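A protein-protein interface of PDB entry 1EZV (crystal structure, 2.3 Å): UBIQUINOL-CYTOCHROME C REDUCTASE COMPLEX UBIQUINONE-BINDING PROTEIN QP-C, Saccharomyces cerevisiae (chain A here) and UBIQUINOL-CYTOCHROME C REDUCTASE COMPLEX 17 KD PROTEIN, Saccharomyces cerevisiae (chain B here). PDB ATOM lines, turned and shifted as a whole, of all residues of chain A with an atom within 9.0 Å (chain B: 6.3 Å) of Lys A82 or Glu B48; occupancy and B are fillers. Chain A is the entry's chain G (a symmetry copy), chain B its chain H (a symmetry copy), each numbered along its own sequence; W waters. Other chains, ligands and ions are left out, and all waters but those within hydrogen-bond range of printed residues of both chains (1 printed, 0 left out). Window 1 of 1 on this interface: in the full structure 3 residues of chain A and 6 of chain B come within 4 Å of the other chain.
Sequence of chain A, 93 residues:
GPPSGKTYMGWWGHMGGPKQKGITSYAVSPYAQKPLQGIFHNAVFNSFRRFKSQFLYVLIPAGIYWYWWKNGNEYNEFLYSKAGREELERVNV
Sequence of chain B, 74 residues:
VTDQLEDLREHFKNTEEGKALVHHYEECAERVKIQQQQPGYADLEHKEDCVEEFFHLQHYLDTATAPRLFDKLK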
ATOM      1  N   ASN A  76       2.359 -23.139  25.742  1.00  0.00           N
ATOM      2  CA  ASN A  76       1.477 -22.013  25.438  1.00  0.00           C
ATOM      3  C   ASN A  76       0.213 -22.528  24.744  1.00  0.00           C
ATOM      4  O   ASN A  76      -0.887 -22.022  24.975  1.00  0.00           O
ATOM      5  CB  ASN A  76       2.209 -21.002  24.534  1.00  0.00           C
ATOM      6  CG  ASN A  76       1.351 -19.795  24.171  1.00  0.00           C
ATOM      7  OD1 ASN A  76       0.760 -19.740  23.098  1.00  0.00           O
ATOM      8  ND2 ASN A  76       1.309 -18.816  25.052  1.00  0.00           N
ATOM      9  N   GLU A  77       0.391 -23.543  23.901  1.00  0.00           N
ATOM     10  CA  GLU A  77      -0.701 -24.180  23.182  1.00  0.00           C
ATOM     11  C   GLU A  77      -1.667 -24.839  24.165  1.00  0.00           C
ATOM     12  O   GLU A  77      -2.876 -24.601  24.119  1.00  0.00           O
ATOM     13  CB  GLU A  77      -0.137 -25.224  22.224  1.00  0.00           C
ATOM     14  CG  GLU A  77      -0.921 -25.382  20.938  1.00  0.00           C
ATOM     15  CD  GLU A  77      -0.202 -26.269  19.933  1.00  0.00           C
ATOM     16  OE1 GLU A  77       0.812 -25.811  19.352  1.00  0.00           O
ATOM     17  OE2 GLU A  77      -0.633 -27.431  19.743  1.00  0.00           O
ATOM     18  N   PHE A  78      -1.118 -25.601  25.105  1.00  0.00           N
ATOM     19  CA  PHE A  78      -1.915 -26.193  26.168  1.00  0.00           C
ATOM     20  C   PHE A  78      -2.696 -25.127  26.941  1.00  0.00           C
ATOM     21  O   PHE A  78      -3.912 -25.216  27.065  1.00  0.00           O
ATOM     22  CB  PHE A  78      -1.012 -26.989  27.115  1.00  0.00           C
ATOM     23  CG  PHE A  78      -1.668 -27.361  28.419  1.00  0.00           C
ATOM     24  CD1 PHE A  78      -2.618 -28.377  28.471  1.00  0.00           C
ATOM     25  CD2 PHE A  78      -1.317 -26.706  29.602  1.00  0.00           C
ATOM     26  CE1 PHE A  78      -3.210 -28.741  29.686  1.00  0.00           C
ATOM     27  CE2 PHE A  78      -1.903 -27.059  30.820  1.00  0.00           C
ATOM     28  CZ  PHE A  78      -2.851 -28.082  30.862  1.00  0.00           C
ATOM     29  N   LEU A  79      -2.014 -24.065  27.356  1.00  0.00           N
ATOM     30  CA  LEU A  79      -2.642 -23.028  28.166  1.00  0.00           C
ATOM     31  C   LEU A  79      -3.892 -22.408  27.524  1.00  0.00           C
ATOM     32  O   LEU A  79      -4.831 -22.035  28.220  1.00  0.00           O
ATOM     33  CB  LEU A  79      -1.628 -21.930  28.487  1.00  0.00           C
ATOM     34  CG  LEU A  79      -0.561 -22.252  29.534  1.00  0.00           C
ATOM     35  CD1 LEU A  79       0.456 -21.116  29.606  1.00  0.00           C
ATOM     36  CD2 LEU A  79      -1.223 -22.435  30.887  1.00  0.00           C
ATOM     37  N   TYR A  80      -3.916 -22.337  26.196  1.00  0.00           N
ATOM     38  CA  TYR A  80      -4.999 -21.657  25.492  1.00  0.00           C
ATOM     39  C   TYR A  80      -5.994 -22.627  24.848  1.00  0.00           C
ATOM     40  O   TYR A  80      -6.933 -22.209  24.166  1.00  0.00           O
ATOM     41  CB  TYR A  80      -4.419 -20.684  24.452  1.00  0.00           C
ATOM     42  CG  TYR A  80      -3.864 -19.416  25.072  1.00  0.00           C
ATOM     43  CD1 TYR A  80      -2.542 -19.357  25.514  1.00  0.00           C
ATOM     44  CD2 TYR A  80      -4.703 -18.337  25.364  1.00  0.00           C
ATOM     45  CE1 TYR A  80      -2.073 -18.270  26.247  1.00  0.00           C
ATOM     46  CE2 TYR A  80      -4.243 -17.244  26.085  1.00  0.00           C
ATOM     47  CZ  TYR A  80      -2.928 -17.221  26.525  1.00  0.00           C
ATOM     48  OH  TYR A  80      -2.462 -16.141  27.229  1.00  0.00           O
ATOM     49  N   SER A  81      -5.811 -23.918  25.109  1.00  0.00           N
ATOM     50  CA  SER A  81      -6.834 -24.918  24.814  1.00  0.00           C
ATOM     51  C   SER A  81      -7.825 -25.023  25.976  1.00  0.00           C
ATOM     52  O   SER A  81      -7.625 -24.418  27.033  1.00  0.00           O
ATOM     53  CB  SER A  81      -6.188 -26.282  24.561  1.00  0.00           C
ATOM     54  OG  SER A  81      -5.614 -26.800  25.749  1.00  0.00           O
ATOM     55  N   LYS A  82      -8.906 -25.773  25.760  1.00  0.00           N
ATOM     56  CA  LYS A  82      -9.926 -25.993  26.786  1.00  0.00           C
ATOM     57  C   LYS A  82      -9.319 -26.618  28.033  1.00  0.00           C
ATOM     58  O   LYS A  82      -9.496 -26.108  29.142  1.00  0.00           O
ATOM     59  CB  LYS A  82     -11.017 -26.918  26.256  1.00  0.00           C
ATOM     60  CG  LYS A  82     -12.244 -26.205  25.738  1.00  0.00           C
ATOM     61  CD  LYS A  82     -13.346 -27.200  25.418  1.00  0.00           C
ATOM     62  CE  LYS A  82     -14.522 -26.499  24.790  1.00  0.00           C
ATOM     63  NZ  LYS A  82     -15.485 -27.462  24.205  1.00  0.00           N
ATOM     64  N   ALA A  83      -8.557 -27.690  27.825  1.00  0.00           N
ATOM     65  CA  ALA A  83      -7.965 -28.468  28.909  1.00  0.00           C
ATOM     66  C   ALA A  83      -7.141 -27.627  29.877  1.00  0.00           C
ATOM     67  O   ALA A  83      -7.036 -27.959  31.062  1.00  0.00           O
ATOM     68  CB  ALA A  83      -7.102 -29.593  28.332  1.00  0.00           C
ATOM     69  N   GLY A  84      -6.606 -26.513  29.385  1.00  0.00           N
ATOM     70  CA  GLY A  84      -5.636 -25.757  30.156  1.00  0.00           C
ATOM     71  C   GLY A  84      -6.117 -24.428  30.700  1.00  0.00           C
ATOM     72  O   GLY A  84      -5.342 -23.715  31.336  1.00  0.00           O
ATOM     73  N   ARG A  85      -7.394 -24.111  30.500  1.00  0.00           N
ATOM     74  CA  ARG A  85      -7.919 -22.800  30.871  1.00  0.00           C
ATOM     75  C   ARG A  85      -7.934 -22.591  32.381  1.00  0.00           C
ATOM     76  O   ARG A  85      -8.000 -21.459  32.860  1.00  0.00           O
ATOM     77  CB  ARG A  85      -9.327 -22.589  30.297  1.00  0.00           C
ATOM     78  CG  ARG A  85     -10.382 -23.558  30.805  1.00  0.00           C
ATOM     79  CD  ARG A  85     -11.792 -22.999  30.623  1.00  0.00           C
ATOM     80  NE  ARG A  85     -11.955 -21.693  31.261  1.00  0.00           N
ATOM     81  CZ  ARG A  85     -11.860 -21.469  32.571  1.00  0.00           C
ATOM     82  NH1 ARG A  85     -11.987 -20.233  33.043  1.00  0.00           N
ATOM     83  NH2 ARG A  85     -11.658 -22.476  33.416  1.00  0.00           N
ATOM     84  N   GLU A  86      -7.809 -23.687  33.119  1.00  0.00           N
ATOM     85  CA  GLU A  86      -7.737 -23.640  34.572  1.00  0.00           C
ATOM     86  C   GLU A  86      -6.328 -23.249  35.006  1.00  0.00           C
ATOM     87  O   GLU A  86      -6.149 -22.329  35.803  1.00  0.00           O
ATOM     88  CB  GLU A  86      -8.115 -25.003  35.155  1.00  0.00           C
ATOM     89  CG  GLU A  86      -8.737 -24.932  36.540  1.00  0.00           C
ATOM     90  CD  GLU A  86      -9.431 -26.225  36.931  1.00  0.00           C
ATOM     91  OE1 GLU A  86      -8.729 -27.241  37.143  1.00  0.00           O
ATOM     92  OE2 GLU A  86     -10.680 -26.224  37.020  1.00  0.00           O
ATOM     93  N   GLU A  87      -5.333 -23.923  34.428  1.00  0.00           N
ATOM     94  CA  GLU A  87      -3.931 -23.553  34.598  1.00  0.00           C
ATOM     95  C   GLU A  87      -3.636 -22.141  34.083  1.00  0.00           C
ATOM     96  O   GLU A  87      -2.861 -21.407  34.693  1.00  0.00           O
ATOM     97  CB  GLU A  87      -3.030 -24.566  33.889  1.00  0.00           C
ATOM     98  CG  GLU A  87      -1.561 -24.169  33.856  1.00  0.00           C
ATOM     99  CD  GLU A  87      -0.655 -25.178  34.525  1.00  0.00           C
ATOM    100  OE1 GLU A  87       0.020 -25.943  33.802  1.00  0.00           O
ATOM    101  OE2 GLU A  87      -0.595 -25.184  35.773  1.00  0.00           O
ATOM    102  N   LEU A  88      -4.290 -21.754  32.989  1.00  0.00           N
ATOM    103  CA  LEU A  88      -4.151 -20.408  32.430  1.00  0.00           C
ATOM    104  C   LEU A  88      -4.542 -19.347  33.456  1.00  0.00           C
ATOM    105  O   LEU A  88      -3.803 -18.394  33.676  1.00  0.00           O
ATOM    106  CB  LEU A  88      -5.007 -20.264  31.161  1.00  0.00           C
ATOM    107  CG  LEU A  88      -4.852 -19.069  30.203  1.00  0.00           C
ATOM    108  CD1 LEU A  88      -5.882 -18.003  30.527  1.00  0.00           C
ATOM    109  CD2 LEU A  88      -3.448 -18.496  30.268  1.00  0.00           C
ATOM    110  N   CYS B  28     -20.135 -32.403  22.500  1.00  0.00           N
ATOM    111  CA  CYS B  28     -19.929 -31.065  23.039  1.00  0.00           C
ATOM    112  C   CYS B  28     -21.199 -30.230  22.926  1.00  0.00           C
ATOM    113  O   CYS B  28     -21.586 -29.552  23.875  1.00  0.00           O
ATOM    114  CB  CYS B  28     -18.780 -30.356  22.311  1.00  0.00           C
ATOM    115  SG  CYS B  28     -18.342 -28.732  23.023  1.00  0.00           S
ATOM    116  N   ARG B  31     -23.815 -31.155  25.510  1.00  0.00           N
ATOM    117  CA  ARG B  31     -23.393 -30.646  26.811  1.00  0.00           C
ATOM    118  C   ARG B  31     -23.694 -29.154  26.975  1.00  0.00           C
ATOM    119  O   ARG B  31     -24.055 -28.706  28.062  1.00  0.00           O
ATOM    120  CB  ARG B  31     -21.894 -30.913  26.994  1.00  0.00           C
ATOM    121  CG  ARG B  31     -21.360 -30.662  28.393  1.00  0.00           C
ATOM    122  CD  ARG B  31     -20.009 -31.345  28.604  1.00  0.00           C
ATOM    123  NE  ARG B  31     -18.962 -30.819  27.725  1.00  0.00           N
ATOM    124  CZ  ARG B  31     -18.331 -31.533  26.795  1.00  0.00           C
ATOM    125  NH1 ARG B  31     -17.388 -30.968  26.050  1.00  0.00           N
ATOM    126  NH2 ARG B  31     -18.654 -32.804  26.591  1.00  0.00           N
ATOM    127  N   VAL B  32     -23.663 -28.418  25.868  1.00  0.00           N
ATOM    128  CA  VAL B  32     -23.842 -26.970  25.900  1.00  0.00           C
ATOM    129  C   VAL B  32     -25.307 -26.551  26.009  1.00  0.00           C
ATOM    130  O   VAL B  32     -25.644 -25.697  26.828  1.00  0.00           O
ATOM    131  CB  VAL B  32     -23.197 -26.301  24.658  1.00  0.00           C
ATOM    132  CG1 VAL B  32     -23.520 -24.811  24.621  1.00  0.00           C
ATOM    133  CG2 VAL B  32     -21.695 -26.497  24.691  1.00  0.00           C
ATOM    134  N   GLN B  35     -26.608 -26.830  29.394  1.00  0.00           N
ATOM    135  CA  GLN B  35     -26.135 -25.760  30.269  1.00  0.00           C
ATOM    136  C   GLN B  35     -26.955 -24.480  30.110  1.00  0.00           C
ATOM    137  O   GLN B  35     -27.072 -23.691  31.048  1.00  0.00           O
ATOM    138  CB  GLN B  35     -24.660 -25.457  29.987  1.00  0.00           C
ATOM    139  CG  GLN B  35     -23.683 -26.494  30.519  1.00  0.00           C
ATOM    140  CD  GLN B  35     -22.232 -26.125  30.248  1.00  0.00           C
ATOM    141  OE1 GLN B  35     -21.892 -24.949  30.101  1.00  0.00           O
ATOM    142  NE2 GLN B  35     -21.367 -27.132  30.188  1.00  0.00           N
ATOM    143  N   TYR B  41     -27.567 -18.863  33.508  1.00  0.00           N
ATOM    144  CA  TYR B  41     -26.699 -18.973  32.341  1.00  0.00           C
ATOM    145  C   TYR B  41     -26.242 -17.599  31.867  1.00  0.00           C
ATOM    146  O   TYR B  41     -25.072 -17.412  31.530  1.00  0.00           O
ATOM    147  CB  TYR B  41     -27.419 -19.703  31.204  1.00  0.00           C
ATOM    148  CG  TYR B  41     -26.542 -19.958  30.000  1.00  0.00           C
ATOM    149  CD1 TYR B  41     -26.785 -19.313  28.787  1.00  0.00           C
ATOM    150  CD2 TYR B  41     -25.438 -20.806  30.084  1.00  0.00           C
ATOM    151  CE1 TYR B  41     -25.949 -19.505  27.689  1.00  0.00           C
ATOM    152  CE2 TYR B  41     -24.596 -21.005  28.993  1.00  0.00           C
ATOM    153  CZ  TYR B  41     -24.857 -20.350  27.798  1.00  0.00           C
ATOM    154  OH  TYR B  41     -24.033 -20.543  26.714  1.00  0.00           O
ATOM    155  N   HIS B  46     -18.482 -18.222  32.593  1.00  0.00           N
ATOM    156  CA  HIS B  46     -17.783 -19.495  32.428  1.00  0.00           C
ATOM    157  C   HIS B  46     -18.521 -20.378  31.419  1.00  0.00           C
ATOM    158  O   HIS B  46     -18.586 -21.601  31.576  1.00  0.00           O
ATOM    159  CB  HIS B  46     -17.680 -20.213  33.780  1.00  0.00           C
ATOM    160  CG  HIS B  46     -16.405 -20.975  33.969  1.00  0.00           C
ATOM    161  ND1 HIS B  46     -16.147 -22.167  33.325  1.00  0.00           N
ATOM    162  CD2 HIS B  46     -15.330 -20.732  34.756  1.00  0.00           C
ATOM    163  CE1 HIS B  46     -14.972 -22.629  33.713  1.00  0.00           C
ATOM    164  NE2 HIS B  46     -14.455 -21.777  34.581  1.00  0.00           N
ATOM    165  N   LYS B  47     -19.065 -19.750  30.380  1.00  0.00           N
ATOM    166  CA  LYS B  47     -19.846 -20.450  29.365  1.00  0.00           C
ATOM    167  C   LYS B  47     -18.942 -21.202  28.394  1.00  0.00           C
ATOM    168  O   LYS B  47     -18.023 -20.627  27.808  1.00  0.00           O
ATOM    169  CB  LYS B  47     -20.719 -19.459  28.588  1.00  0.00           C
ATOM    170  CG  LYS B  47     -21.518 -18.497  29.461  1.00  0.00           C
ATOM    171  CD  LYS B  47     -22.242 -17.455  28.616  1.00  0.00           C
ATOM    172  CE  LYS B  47     -22.177 -16.068  29.249  1.00  0.00           C
ATOM    173  NZ  LYS B  47     -23.059 -15.937  30.442  1.00  0.00           N
ATOM    174  N   GLU B  48     -19.195 -22.497  28.247  1.00  0.00           N
ATOM    175  CA  GLU B  48     -18.434 -23.331  27.329  1.00  0.00           C
ATOM    176  C   GLU B  48     -19.004 -23.229  25.917  1.00  0.00           C
ATOM    177  O   GLU B  48     -20.221 -23.144  25.732  1.00  0.00           O
ATOM    178  CB  GLU B  48     -18.463 -24.788  27.794  1.00  0.00           C
ATOM    179  CG  GLU B  48     -17.578 -25.723  26.975  1.00  0.00           C
ATOM    180  CD  GLU B  48     -17.684 -27.178  27.399  1.00  0.00           C
ATOM    181  OE1 GLU B  48     -18.486 -27.492  28.306  1.00  0.00           O
ATOM    182  OE2 GLU B  48     -16.962 -28.018  26.819  1.00  0.00           O
ATOM    183  N   ASP B  49     -18.111 -23.152  24.932  1.00  0.00           N
ATOM    184  CA  ASP B  49     -18.499 -23.266  23.532  1.00  0.00           C
ATOM    185  C   ASP B  49     -17.794 -24.452  22.893  1.00  0.00           C
ATOM    186  O   ASP B  49     -16.971 -25.104  23.526  1.00  0.00           O
ATOM    187  CB  ASP B  49     -18.182 -21.974  22.764  1.00  0.00           C
ATOM    188  CG  ASP B  49     -16.711 -21.596  22.824  1.00  0.00           C
ATOM    189  OD1 ASP B  49     -16.406 -20.530  23.404  1.00  0.00           O
ATOM    190  OD2 ASP B  49     -15.869 -22.326  22.249  1.00  0.00           O
ATOM    191  N   CYS B  50     -18.101 -24.719  21.631  1.00  0.00           N
ATOM    192  CA  CYS B  50     -17.569 -25.897  20.968  1.00  0.00           C
ATOM    193  C   CYS B  50     -16.749 -25.553  19.721  1.00  0.00           C
ATOM    194  O   CYS B  50     -16.575 -26.392  18.826  1.00  0.00           O
ATOM    195  CB  CYS B  50     -18.717 -26.859  20.640  1.00  0.00           C
ATOM    196  SG  CYS B  50     -19.623 -27.431  22.122  1.00  0.00           S
ATOM    197  N   VAL B  51     -16.125 -24.372  19.749  1.00  0.00           N
ATOM    198  CA  VAL B  51     -15.253 -23.912  18.667  1.00  0.00           C
ATOM    199  C   VAL B  51     -14.077 -24.865  18.470  1.00  0.00           C
ATOM    200  O   VAL B  51     -13.815 -25.316  17.360  1.00  0.00           O
ATOM    201  CB  VAL B  51     -14.707 -22.490  18.949  1.00  0.00           C
ATOM    202  CG1 VAL B  51     -13.740 -22.068  17.854  1.00  0.00           C
ATOM    203  CG2 VAL B  51     -15.843 -21.497  19.027  1.00  0.00           C
ATOM    204  N   GLU B  52     -13.462 -25.264  19.576  1.00  0.00           N
ATOM    205  CA  GLU B  52     -12.307 -26.147  19.551  1.00  0.00           C
ATOM    206  C   GLU B  52     -12.631 -27.453  18.832  1.00  0.00           C
ATOM    207  O   GLU B  52     -11.973 -27.806  17.855  1.00  0.00           O
ATOM    208  CB  GLU B  52     -11.842 -26.424  20.979  1.00  0.00           C
ATOM    209  CG  GLU B  52     -10.558 -27.221  21.077  1.00  0.00           C
ATOM    210  CD  GLU B  52      -9.889 -27.088  22.435  1.00  0.00           C
ATOM    211  OE1 GLU B  52      -9.432 -28.120  22.969  1.00  0.00           O
ATOM    212  OE2 GLU B  52      -9.804 -25.954  22.964  1.00  0.00           O
ATOM    213  N   GLU B  53     -13.711 -28.107  19.259  1.00  0.00           N
ATOM    214  CA  GLU B  53     -14.158 -29.359  18.651  1.00  0.00           C
ATOM    215  C   GLU B  53     -14.587 -29.143  17.205  1.00  0.00           C
ATOM    216  O   GLU B  53     -14.299 -29.967  16.336  1.00  0.00           O
ATOM    217  CB  GLU B  53     -15.321 -29.959  19.448  1.00  0.00           C
ATOM    218  CG  GLU B  53     -14.939 -30.494  20.827  1.00  0.00           C
ATOM    219  CD  GLU B  53     -14.856 -29.411  21.892  1.00  0.00           C
ATOM    220  OE1 GLU B  53     -15.291 -28.267  21.632  1.00  0.00           O
ATOM    221  OE2 GLU B  53     -14.365 -29.713  23.002  1.00  0.00           O
HETATM  222  O   HOH W   1      -8.440 -28.854  25.428  1.00  0.00           O
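The side-chain carboxylate of Glu B48 lies within salt-bridge range of the side-chain amino group of Lys A82, 3.1 Å away.
The guanidinium group (NH2) of Arg A85 sits at hydrogen-bond distance from a ring nitrogen (NE2) of His B46 (3.1 Å).
The side-chain amino group of Lys A82 is in hydrogen-bond range of the side-chain sulfur of Cys B28.
OE1 of Glu B53 lies within salt-bridge range of NZ of Lys A82.
OE2 of Glu B52 sits at hydrogen-bond distance from N of Lys A82 (2.9 Å).
The backbone carbonyl oxygen (O) of Asp B49 is in hydrogen-bond range of the side-chain amino group (NZ) of Lys A82.
The backbone carbonyl oxygen (O) of Phe A78 is in hydrogen-bond range of the side-chain hydroxyl (OG) of Ser A81 (2.7 Å).
The side-chain sulfur (SG) of Cys B28 is disulfide-bonded to the side-chain sulfur (SG) of Cys B50, at 2.0 Å.
OD2 of Asp B49 sits at hydrogen-bond distance from N of Val B51, 3.2 Å away.
The side-chain carboxylate of Glu B48 lies within hydrogen-bond range of the side-chain amide nitrogen of Gln B35 (3.5 Å).
NH1 of Arg B31 lies within salt-bridge range of OE2 of Glu B48.
Of the 13 printed residues of chain A, 3 touch a printed residue of chain B.
Of the 13 printed residues of chain B, 6 touch a printed residue of chain A.
Hydrophobic or aromatic side chains of chain B that line the printed part of chain A: His B46.
Along chain B the printed residues that touch a printed residue of chain A span positions 28 to 53.
Among the printed residues, 7 pairs touch across the chains.
Lys A82 touches just these residues of chain B: Cys B28, Glu B48, Asp B49, Glu B52 and Glu B53.
Of chain A, only Lys A82 comes within 4 Å of Asp B49.
Printed residues of chain A within 4 Å of His B46: Arg A85.
Printed residues of chain B within 4 Å of Arg A85: His B46 (3.1 Å).
Tyr B41 touches none of the printed residues of chain A.
Leu A88 touches none of the printed residues of chain B.
The nearest residue of chain A that does not touch Glu B48 is Arg A85 (7.4 Å).
The nearest printed residue of chain A that does not touch Cys B28 is Ala A83 (10.9 Å).
Water W1 lies within hydrogen-bond range of N of Ala A83 (2.7 Å), OE1 of Glu B52 (2.8 Å) and N of Lys A82 (3.1 Å).
Among the printed residues, pairs that only touch across the chains: Ser A81 with Glu B52 (3.6 Å).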
